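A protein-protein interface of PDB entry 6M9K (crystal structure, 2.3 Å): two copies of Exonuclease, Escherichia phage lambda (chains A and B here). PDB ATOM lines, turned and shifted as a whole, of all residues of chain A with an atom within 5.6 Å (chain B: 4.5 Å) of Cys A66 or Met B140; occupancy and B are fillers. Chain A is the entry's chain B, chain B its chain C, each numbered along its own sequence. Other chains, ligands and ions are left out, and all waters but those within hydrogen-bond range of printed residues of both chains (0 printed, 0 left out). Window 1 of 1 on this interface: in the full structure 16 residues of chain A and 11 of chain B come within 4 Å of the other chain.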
ATOM      1  N   HIS A  59       0.771  -6.538  15.199  1.00  0.00           N
ATOM      2  CA  HIS A  59       2.067  -7.015  14.716  1.00  0.00           C
ATOM      3  C   HIS A  59       3.199  -6.778  15.721  1.00  0.00           C
ATOM      4  O   HIS A  59       4.140  -7.583  15.820  1.00  0.00           O
ATOM      5  CB  HIS A  59       2.415  -6.355  13.379  1.00  0.00           C
ATOM      6  CG  HIS A  59       1.517  -6.753  12.253  1.00  0.00           C
ATOM      7  ND1 HIS A  59       1.094  -5.862  11.292  1.00  0.00           N
ATOM      8  CD2 HIS A  59       0.963  -7.945  11.927  1.00  0.00           C
ATOM      9  CE1 HIS A  59       0.318  -6.486  10.423  1.00  0.00           C
ATOM     10  NE2 HIS A  59       0.222  -7.751  10.784  1.00  0.00           N
ATOM     11  N   LEU A  61       2.851  -6.591  19.048  1.00  0.00           N
ATOM     12  CA  LEU A  61       2.639  -7.501  20.148  1.00  0.00           C
ATOM     13  C   LEU A  61       3.059  -8.924  19.748  1.00  0.00           C
ATOM     14  O   LEU A  61       3.730  -9.626  20.516  1.00  0.00           O
ATOM     15  CB  LEU A  61       1.171  -7.445  20.572  1.00  0.00           C
ATOM     16  CG  LEU A  61       0.794  -7.625  22.043  1.00  0.00           C
ATOM     17  CD1 LEU A  61       1.597  -6.691  22.929  1.00  0.00           C
ATOM     18  CD2 LEU A  61      -0.711  -7.388  22.219  1.00  0.00           C
ATOM     19  N   LEU A  62       2.700  -9.335  18.530  1.00  0.00           N
ATOM     20  CA  LEU A  62       3.135 -10.638  18.013  1.00  0.00           C
ATOM     21  C   LEU A  62       4.645 -10.736  17.986  1.00  0.00           C
ATOM     22  O   LEU A  62       5.211 -11.743  18.422  1.00  0.00           O
ATOM     23  CB  LEU A  62       2.567 -10.905  16.624  1.00  0.00           C
ATOM     24  CG  LEU A  62       1.048 -11.105  16.612  1.00  0.00           C
ATOM     25  CD1 LEU A  62       0.513 -11.012  15.196  1.00  0.00           C
ATOM     26  CD2 LEU A  62       0.655 -12.419  17.252  1.00  0.00           C
ATOM     27  N   ALA A  63       5.301  -9.684  17.503  1.00  0.00           N
ATOM     28  CA  ALA A  63       6.769  -9.661  17.502  1.00  0.00           C
ATOM     29  C   ALA A  63       7.394  -9.794  18.907  1.00  0.00           C
ATOM     30  O   ALA A  63       8.497 -10.333  19.049  1.00  0.00           O
ATOM     31  CB  ALA A  63       7.290  -8.415  16.802  1.00  0.00           C
ATOM     32  N   GLU A  64       6.715  -9.302  19.933  1.00  0.00           N
ATOM     33  CA  GLU A  64       7.249  -9.384  21.292  1.00  0.00           C
ATOM     34  C   GLU A  64       7.330 -10.828  21.734  1.00  0.00           C
ATOM     35  O   GLU A  64       8.342 -11.243  22.308  1.00  0.00           O
ATOM     36  CB  GLU A  64       6.417  -8.571  22.289  1.00  0.00           C
ATOM     37  CG  GLU A  64       6.555  -7.074  22.095  1.00  0.00           C
ATOM     38  CD  GLU A  64       5.757  -6.241  23.074  1.00  0.00           C
ATOM     39  OE1 GLU A  64       5.149  -6.802  24.013  1.00  0.00           O
ATOM     40  OE2 GLU A  64       5.758  -5.006  22.893  1.00  0.00           O
ATOM     41  N   VAL A  65       6.277 -11.587  21.437  1.00  0.00           N
ATOM     42  CA  VAL A  65       6.243 -13.018  21.732  1.00  0.00           C
ATOM     43  C   VAL A  65       7.399 -13.755  21.045  1.00  0.00           C
ATOM     44  O   VAL A  65       8.089 -14.563  21.676  1.00  0.00           O
ATOM     45  CB  VAL A  65       4.913 -13.658  21.304  1.00  0.00           C
ATOM     46  CG1 VAL A  65       4.939 -15.171  21.542  1.00  0.00           C
ATOM     47  CG2 VAL A  65       3.756 -13.031  22.068  1.00  0.00           C
ATOM     48  N   CYS A  66       7.613 -13.445  19.769  1.00  0.00           N
ATOM     49  CA  CYS A  66       8.562 -14.174  18.934  1.00  0.00           C
ATOM     50  C   CYS A  66      10.006 -13.721  19.026  1.00  0.00           C
ATOM     51  O   CYS A  66      10.886 -14.463  18.568  1.00  0.00           O
ATOM     52  CB  CYS A  66       8.116 -14.117  17.475  1.00  0.00           C
ATOM     53  SG  CYS A  66       6.426 -14.692  17.256  1.00  0.00           S
ATOM     54  N   THR A  67      10.245 -12.503  19.544  1.00  0.00           N
ATOM     55  CA  THR A  67      11.605 -11.979  19.784  1.00  0.00           C
ATOM     56  C   THR A  67      11.991 -11.935  21.273  1.00  0.00           C
ATOM     57  O   THR A  67      13.163 -11.879  21.606  1.00  0.00           O
ATOM     58  CB  THR A  67      11.797 -10.536  19.211  1.00  0.00           C
ATOM     59  OG1 THR A  67      10.992  -9.591  19.942  1.00  0.00           O
ATOM     60  CG2 THR A  67      11.442 -10.464  17.727  1.00  0.00           C
ATOM     61  N   GLY A  68      11.006 -11.917  22.163  1.00  0.00           N
ATOM     62  CA  GLY A  68      11.252 -11.643  23.571  1.00  0.00           C
ATOM     63  C   GLY A  68      11.868 -10.282  23.879  1.00  0.00           C
ATOM     64  O   GLY A  68      12.599 -10.154  24.858  1.00  0.00           O
ATOM     65  N   LEU A 214       0.055 -16.575  15.650  1.00  0.00           N
ATOM     66  CA  LEU A 214       1.172 -17.286  16.292  1.00  0.00           C
ATOM     67  C   LEU A 214       1.264 -18.752  15.840  1.00  0.00           C
ATOM     68  O   LEU A 214       2.349 -19.230  15.511  1.00  0.00           O
ATOM     69  CB  LEU A 214       1.090 -17.198  17.823  1.00  0.00           C
ATOM     70  CG  LEU A 214       1.415 -15.823  18.438  1.00  0.00           C
ATOM     71  CD1 LEU A 214       0.947 -15.754  19.882  1.00  0.00           C
ATOM     72  CD2 LEU A 214       2.889 -15.462  18.364  1.00  0.00           C
ATOM     73  N   ILE A 217       2.920 -19.440  12.399  1.00  0.00           N
ATOM     74  CA  ILE A 217       4.388 -19.433  12.323  1.00  0.00           C
ATOM     75  C   ILE A 217       5.050 -20.303  13.396  1.00  0.00           C
ATOM     76  O   ILE A 217       6.247 -20.164  13.657  1.00  0.00           O
ATOM     77  CB  ILE A 217       4.958 -17.992  12.335  1.00  0.00           C
ATOM     78  CG1 ILE A 217       4.567 -17.210  13.598  1.00  0.00           C
ATOM     79  CG2 ILE A 217       4.477 -17.246  11.111  1.00  0.00           C
ATOM     80  CD1 ILE A 217       5.272 -15.871  13.718  1.00  0.00           C
ATOM     81  N   PHE A 219       4.471 -20.636  16.760  1.00  0.00           N
ATOM     82  CA  PHE A 219       4.704 -20.039  18.073  1.00  0.00           C
ATOM     83  C   PHE A 219       3.456 -20.210  18.937  1.00  0.00           C
ATOM     84  O   PHE A 219       2.347 -20.347  18.422  1.00  0.00           O
ATOM     85  CB  PHE A 219       5.085 -18.558  17.929  1.00  0.00           C
ATOM     86  CG  PHE A 219       6.571 -18.312  17.705  1.00  0.00           C
ATOM     87  CD1 PHE A 219       7.117 -18.288  16.417  1.00  0.00           C
ATOM     88  CD2 PHE A 219       7.418 -18.071  18.779  1.00  0.00           C
ATOM     89  CE1 PHE A 219       8.464 -18.056  16.214  1.00  0.00           C
ATOM     90  CE2 PHE A 219       8.768 -17.833  18.578  1.00  0.00           C
ATOM     91  CZ  PHE A 219       9.294 -17.825  17.295  1.00  0.00           C
ATOM     92  N   SER B 136      10.722  -5.178  14.317  1.00  0.00           N
ATOM     93  CA  SER B 136      10.213  -6.546  14.203  1.00  0.00           C
ATOM     94  C   SER B 136       8.744  -6.542  13.848  1.00  0.00           C
ATOM     95  O   SER B 136       8.262  -7.448  13.181  1.00  0.00           O
ATOM     96  CB  SER B 136      10.446  -7.320  15.500  1.00  0.00           C
ATOM     97  OG  SER B 136      11.817  -7.308  15.841  1.00  0.00           O
ATOM     98  N   ARG B 137       8.031  -5.523  14.307  1.00  0.00           N
ATOM     99  CA  ARG B 137       6.662  -5.275  13.861  1.00  0.00           C
ATOM    100  C   ARG B 137       6.518  -5.390  12.330  1.00  0.00           C
ATOM    101  O   ARG B 137       5.629  -6.094  11.846  1.00  0.00           O
ATOM    102  CB  ARG B 137       6.200  -3.881  14.311  1.00  0.00           C
ATOM    103  CG  ARG B 137       4.795  -3.506  13.829  1.00  0.00           C
ATOM    104  CD  ARG B 137       4.531  -2.001  13.758  1.00  0.00           C
ATOM    105  NE  ARG B 137       5.406  -1.288  12.816  1.00  0.00           N
ATOM    106  CZ  ARG B 137       6.101  -0.170  13.070  1.00  0.00           C
ATOM    107  NH1 ARG B 137       6.064   0.431  14.256  1.00  0.00           N
ATOM    108  NH2 ARG B 137       6.857   0.358  12.117  1.00  0.00           N
ATOM    109  N   ASP B 138       7.358  -4.675  11.586  1.00  0.00           N
ATOM    110  CA  ASP B 138       7.287  -4.709  10.120  1.00  0.00           C
ATOM    111  C   ASP B 138       7.692  -6.049   9.535  1.00  0.00           C
ATOM    112  O   ASP B 138       7.150  -6.462   8.510  1.00  0.00           O
ATOM    113  CB  ASP B 138       8.122  -3.590   9.488  1.00  0.00           C
ATOM    114  CG  ASP B 138       7.428  -2.245   9.554  1.00  0.00           C
ATOM    115  OD1 ASP B 138       6.272  -2.178  10.013  1.00  0.00           O
ATOM    116  OD2 ASP B 138       8.040  -1.246   9.145  1.00  0.00           O
ATOM    117  N   PHE B 139       8.642  -6.717  10.185  1.00  0.00           N
ATOM    118  CA  PHE B 139       8.976  -8.069   9.816  1.00  0.00           C
ATOM    119  C   PHE B 139       7.761  -8.985   9.949  1.00  0.00           C
ATOM    120  O   PHE B 139       7.487  -9.782   9.053  1.00  0.00           O
ATOM    121  CB  PHE B 139      10.139  -8.643  10.632  1.00  0.00           C
ATOM    122  CG  PHE B 139      10.515 -10.021  10.188  1.00  0.00           C
ATOM    123  CD1 PHE B 139      11.320 -10.201   9.064  1.00  0.00           C
ATOM    124  CD2 PHE B 139       9.983 -11.143  10.821  1.00  0.00           C
ATOM    125  CE1 PHE B 139      11.639 -11.474   8.617  1.00  0.00           C
ATOM    126  CE2 PHE B 139      10.299 -12.416  10.376  1.00  0.00           C
ATOM    127  CZ  PHE B 139      11.125 -12.580   9.272  1.00  0.00           C
ATOM    128  N   MET B 140       7.049  -8.855  11.062  1.00  0.00           N
ATOM    129  CA  MET B 140       5.919  -9.729  11.370  1.00  0.00           C
ATOM    130  C   MET B 140       4.804  -9.544  10.377  1.00  0.00           C
ATOM    131  O   MET B 140       4.118 -10.506  10.047  1.00  0.00           O
ATOM    132  CB  MET B 140       5.388  -9.446  12.775  1.00  0.00           C
ATOM    133  CG  MET B 140       4.268 -10.352  13.240  1.00  0.00           C
ATOM    134  SD  MET B 140       4.676 -12.106  13.326  1.00  0.00           S
ATOM    135  CE  MET B 140       6.148 -12.106  14.332  1.00  0.00           C
ATOM    136  N   LYS B 141       4.626  -8.307   9.920  1.00  0.00           N
ATOM    137  CA  LYS B 141       3.639  -7.986   8.900  1.00  0.00           C
ATOM    138  C   LYS B 141       3.924  -8.756   7.613  1.00  0.00           C
ATOM    139  O   LYS B 141       3.033  -9.356   7.022  1.00  0.00           O
ATOM    140  CB  LYS B 141       3.628  -6.479   8.630  1.00  0.00           C
ATOM    141  CG  LYS B 141       2.551  -6.053   7.649  1.00  0.00           C
ATOM    142  CD  LYS B 141       2.512  -4.547   7.453  1.00  0.00           C
ATOM    143  CE  LYS B 141       1.433  -4.150   6.450  1.00  0.00           C
ATOM    144  NZ  LYS B 141       1.720  -2.796   5.912  1.00  0.00           N
ATOM    145  N   PHE B 142       5.178  -8.747   7.192  1.00  0.00           N
ATOM    146  CA  PHE B 142       5.544  -9.437   5.979  1.00  0.00           C
ATOM    147  C   PHE B 142       5.411 -10.954   6.148  1.00  0.00           C
ATOM    148  O   PHE B 142       4.827 -11.635   5.291  1.00  0.00           O
ATOM    149  CB  PHE B 142       6.957  -9.069   5.532  1.00  0.00           C
ATOM    150  CG  PHE B 142       7.423  -9.871   4.368  1.00  0.00           C
ATOM    151  CD1 PHE B 142       6.706  -9.859   3.185  1.00  0.00           C
ATOM    152  CD2 PHE B 142       8.535 -10.684   4.470  1.00  0.00           C
ATOM    153  CE1 PHE B 142       7.116 -10.622   2.112  1.00  0.00           C
ATOM    154  CE2 PHE B 142       8.968 -11.436   3.393  1.00  0.00           C
ATOM    155  CZ  PHE B 142       8.253 -11.411   2.215  1.00  0.00           C
ATOM    156  N   ARG B 143       5.935 -11.460   7.265  1.00  0.00           N
ATOM    157  CA  ARG B 143       5.914 -12.884   7.585  1.00  0.00           C
ATOM    158  C   ARG B 143       4.506 -13.511   7.537  1.00  0.00           C
ATOM    159  O   ARG B 143       4.344 -14.631   7.069  1.00  0.00           O
ATOM    160  CB  ARG B 143       6.585 -13.117   8.953  1.00  0.00           C
ATOM    161  CG  ARG B 143       6.795 -14.571   9.356  1.00  0.00           C
ATOM    162  CD  ARG B 143       7.663 -15.345   8.368  1.00  0.00           C
ATOM    163  NE  ARG B 143       7.650 -16.777   8.631  1.00  0.00           N
ATOM    164  CZ  ARG B 143       6.633 -17.602   8.379  1.00  0.00           C
ATOM    165  NH1 ARG B 143       5.492 -17.168   7.853  1.00  0.00           N
ATOM    166  NH2 ARG B 143       6.747 -18.888   8.688  1.00  0.00           N
ATOM    167  N   LEU B 144       3.494 -12.772   7.967  1.00  0.00           N
ATOM    168  CA  LEU B 144       2.132 -13.304   8.024  1.00  0.00           C
ATOM    169  C   LEU B 144       1.338 -13.122   6.741  1.00  0.00           C
ATOM    170  O   LEU B 144       0.662 -14.033   6.301  1.00  0.00           O
ATOM    171  CB  LEU B 144       1.369 -12.642   9.172  1.00  0.00           C
ATOM    172  CG  LEU B 144       1.964 -12.887  10.558  1.00  0.00           C
ATOM    173  CD1 LEU B 144       1.369 -11.907  11.555  1.00  0.00           C
ATOM    174  CD2 LEU B 144       1.745 -14.330  11.008  1.00  0.00           C
ATOM    175  N   ARG B 178      16.539 -10.594  15.399  1.00  0.00           N
ATOM    176  CA  ARG B 178      15.931 -10.652  16.731  1.00  0.00           C
ATOM    177  C   ARG B 178      14.895 -11.764  16.869  1.00  0.00           C
ATOM    178  O   ARG B 178      14.537 -12.118  17.987  1.00  0.00           O
ATOM    179  CB  ARG B 178      15.260  -9.300  17.087  1.00  0.00           C
ATOM    180  CG  ARG B 178      16.231  -8.125  17.200  1.00  0.00           C
ATOM    181  CD  ARG B 178      15.581  -6.779  16.892  1.00  0.00           C
ATOM    182  NE  ARG B 178      15.088  -6.712  15.518  1.00  0.00           N
ATOM    183  CZ  ARG B 178      14.631  -5.615  14.916  1.00  0.00           C
ATOM    184  NH1 ARG B 178      14.628  -4.439  15.534  1.00  0.00           N
ATOM    185  NH2 ARG B 178      14.197  -5.690  13.657  1.00  0.00           N
ATOM    186  N   MET B 179      14.390 -12.282  15.749  1.00  0.00           N
ATOM    187  CA  MET B 179      13.386 -13.339  15.774  1.00  0.00           C
ATOM    188  C   MET B 179      13.990 -14.676  16.252  1.00  0.00           C
ATOM    189  O   MET B 179      15.007 -15.132  15.721  1.00  0.00           O
ATOM    190  CB  MET B 179      12.766 -13.505  14.381  1.00  0.00           C
ATOM    191  CG  MET B 179      11.801 -12.394  13.976  1.00  0.00           C
ATOM    192  SD  MET B 179      10.224 -12.509  14.837  1.00  0.00           S
ATOM    193  CE  MET B 179       9.465 -13.933  14.061  1.00  0.00           C
ATOM    194  N   LYS B 180      13.361 -15.297  17.246  1.00  0.00           N
ATOM    195  CA  LYS B 180      13.881 -16.535  17.851  1.00  0.00           C
ATOM    196  C   LYS B 180      13.838 -17.725  16.883  1.00  0.00           C
ATOM    197  O   LYS B 180      14.723 -18.576  16.885  1.00  0.00           O
ATOM    198  CB  LYS B 180      13.141 -16.832  19.171  1.00  0.00           C
ATOM    199  CG  LYS B 180      13.501 -15.793  20.237  1.00  0.00           C
ATOM    200  CD  LYS B 180      13.118 -16.168  21.660  1.00  0.00           C
ATOM    201  CE  LYS B 180      11.729 -15.694  22.042  1.00  0.00           C
ATOM    202  NZ  LYS B 180      11.577 -15.572  23.521  1.00  0.00           N
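The side-chain sulfur (SG) of Cys A66 is in hydrogen-bond range of the backbone carbonyl oxygen (O) of Leu A62 (3.4 Å).
O of Ala A63 is in hydrogen-bond range of OG1 of Thr A67 (2.8 Å).
The side-chain hydroxyl of Ser B136 sits at hydrogen-bond distance from the guanidinium group of Arg B178 (3.3 Å).
OD1 of Asp B138 is in salt-bridge range of NE of Arg B137, at 3.1 Å.
No position is printed for both chains.
Hydrophobic or aromatic side chains of chain A within 4 Å of the printed part of chain B: His A59, Leu A62, Ala A63 and Ile A217.
Among the printed residues, no Asp or Glu carboxylate lies within 4 Å of a Lys or Arg side-chain nitrogen of the other chain.
Met B140 touches His A59 (CB to O, 3.8 Å).
Lys B141 touches His A59.
Leu B144 touches Leu A62.
CB of Ala A63 touches CB of Ser B136 (3.6 Å).
Ala A63 touches Arg B137 (CB to N, 3.9 Å).
CE of Met B179 touches CB of Cys A66, at 3.7 Å.
CG2 of Thr A67 touches OG of Ser B136 (3.7 Å).
Lys B180 touches Gly A68 (CE to N, 3.8 Å).
Met B140 touches Ile A217.
Ile A217 touches Leu B144 (CG2 to CD2, 3.997 Å).
The backbone carbonyl oxygen (O) of Cys A66 lies within hydrogen-bond range of the backbone NH (N) of Lys B180 (2.9 Å).
Of the printed residues of chain B, Cys A66 touches Met B140, Met B179 and Lys B180.
Of chain A, only His A59, Leu A62, Cys A66 and Ile A217 come within 4 Å of Met B140.
Of the printed residues of chain B, Gly A68 touches Lys B180.
Of the printed residues of chain B, Thr A67 touches Ser B136, Arg B178, Met B179 and Lys B180.
Of the printed residues of chain A, Arg B143 touches Ile A217 (3.4 Å).
Phe A219 touches none of the printed residues of chain B.
Phe B142 touches none of the printed residues of chain A.
The nearest residue of chain B that does not touch Cys A66 is Arg B178 (4.4 Å).
The nearest printed residue of chain B that does not touch His A59 is Leu B144 (4.0001 Å).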
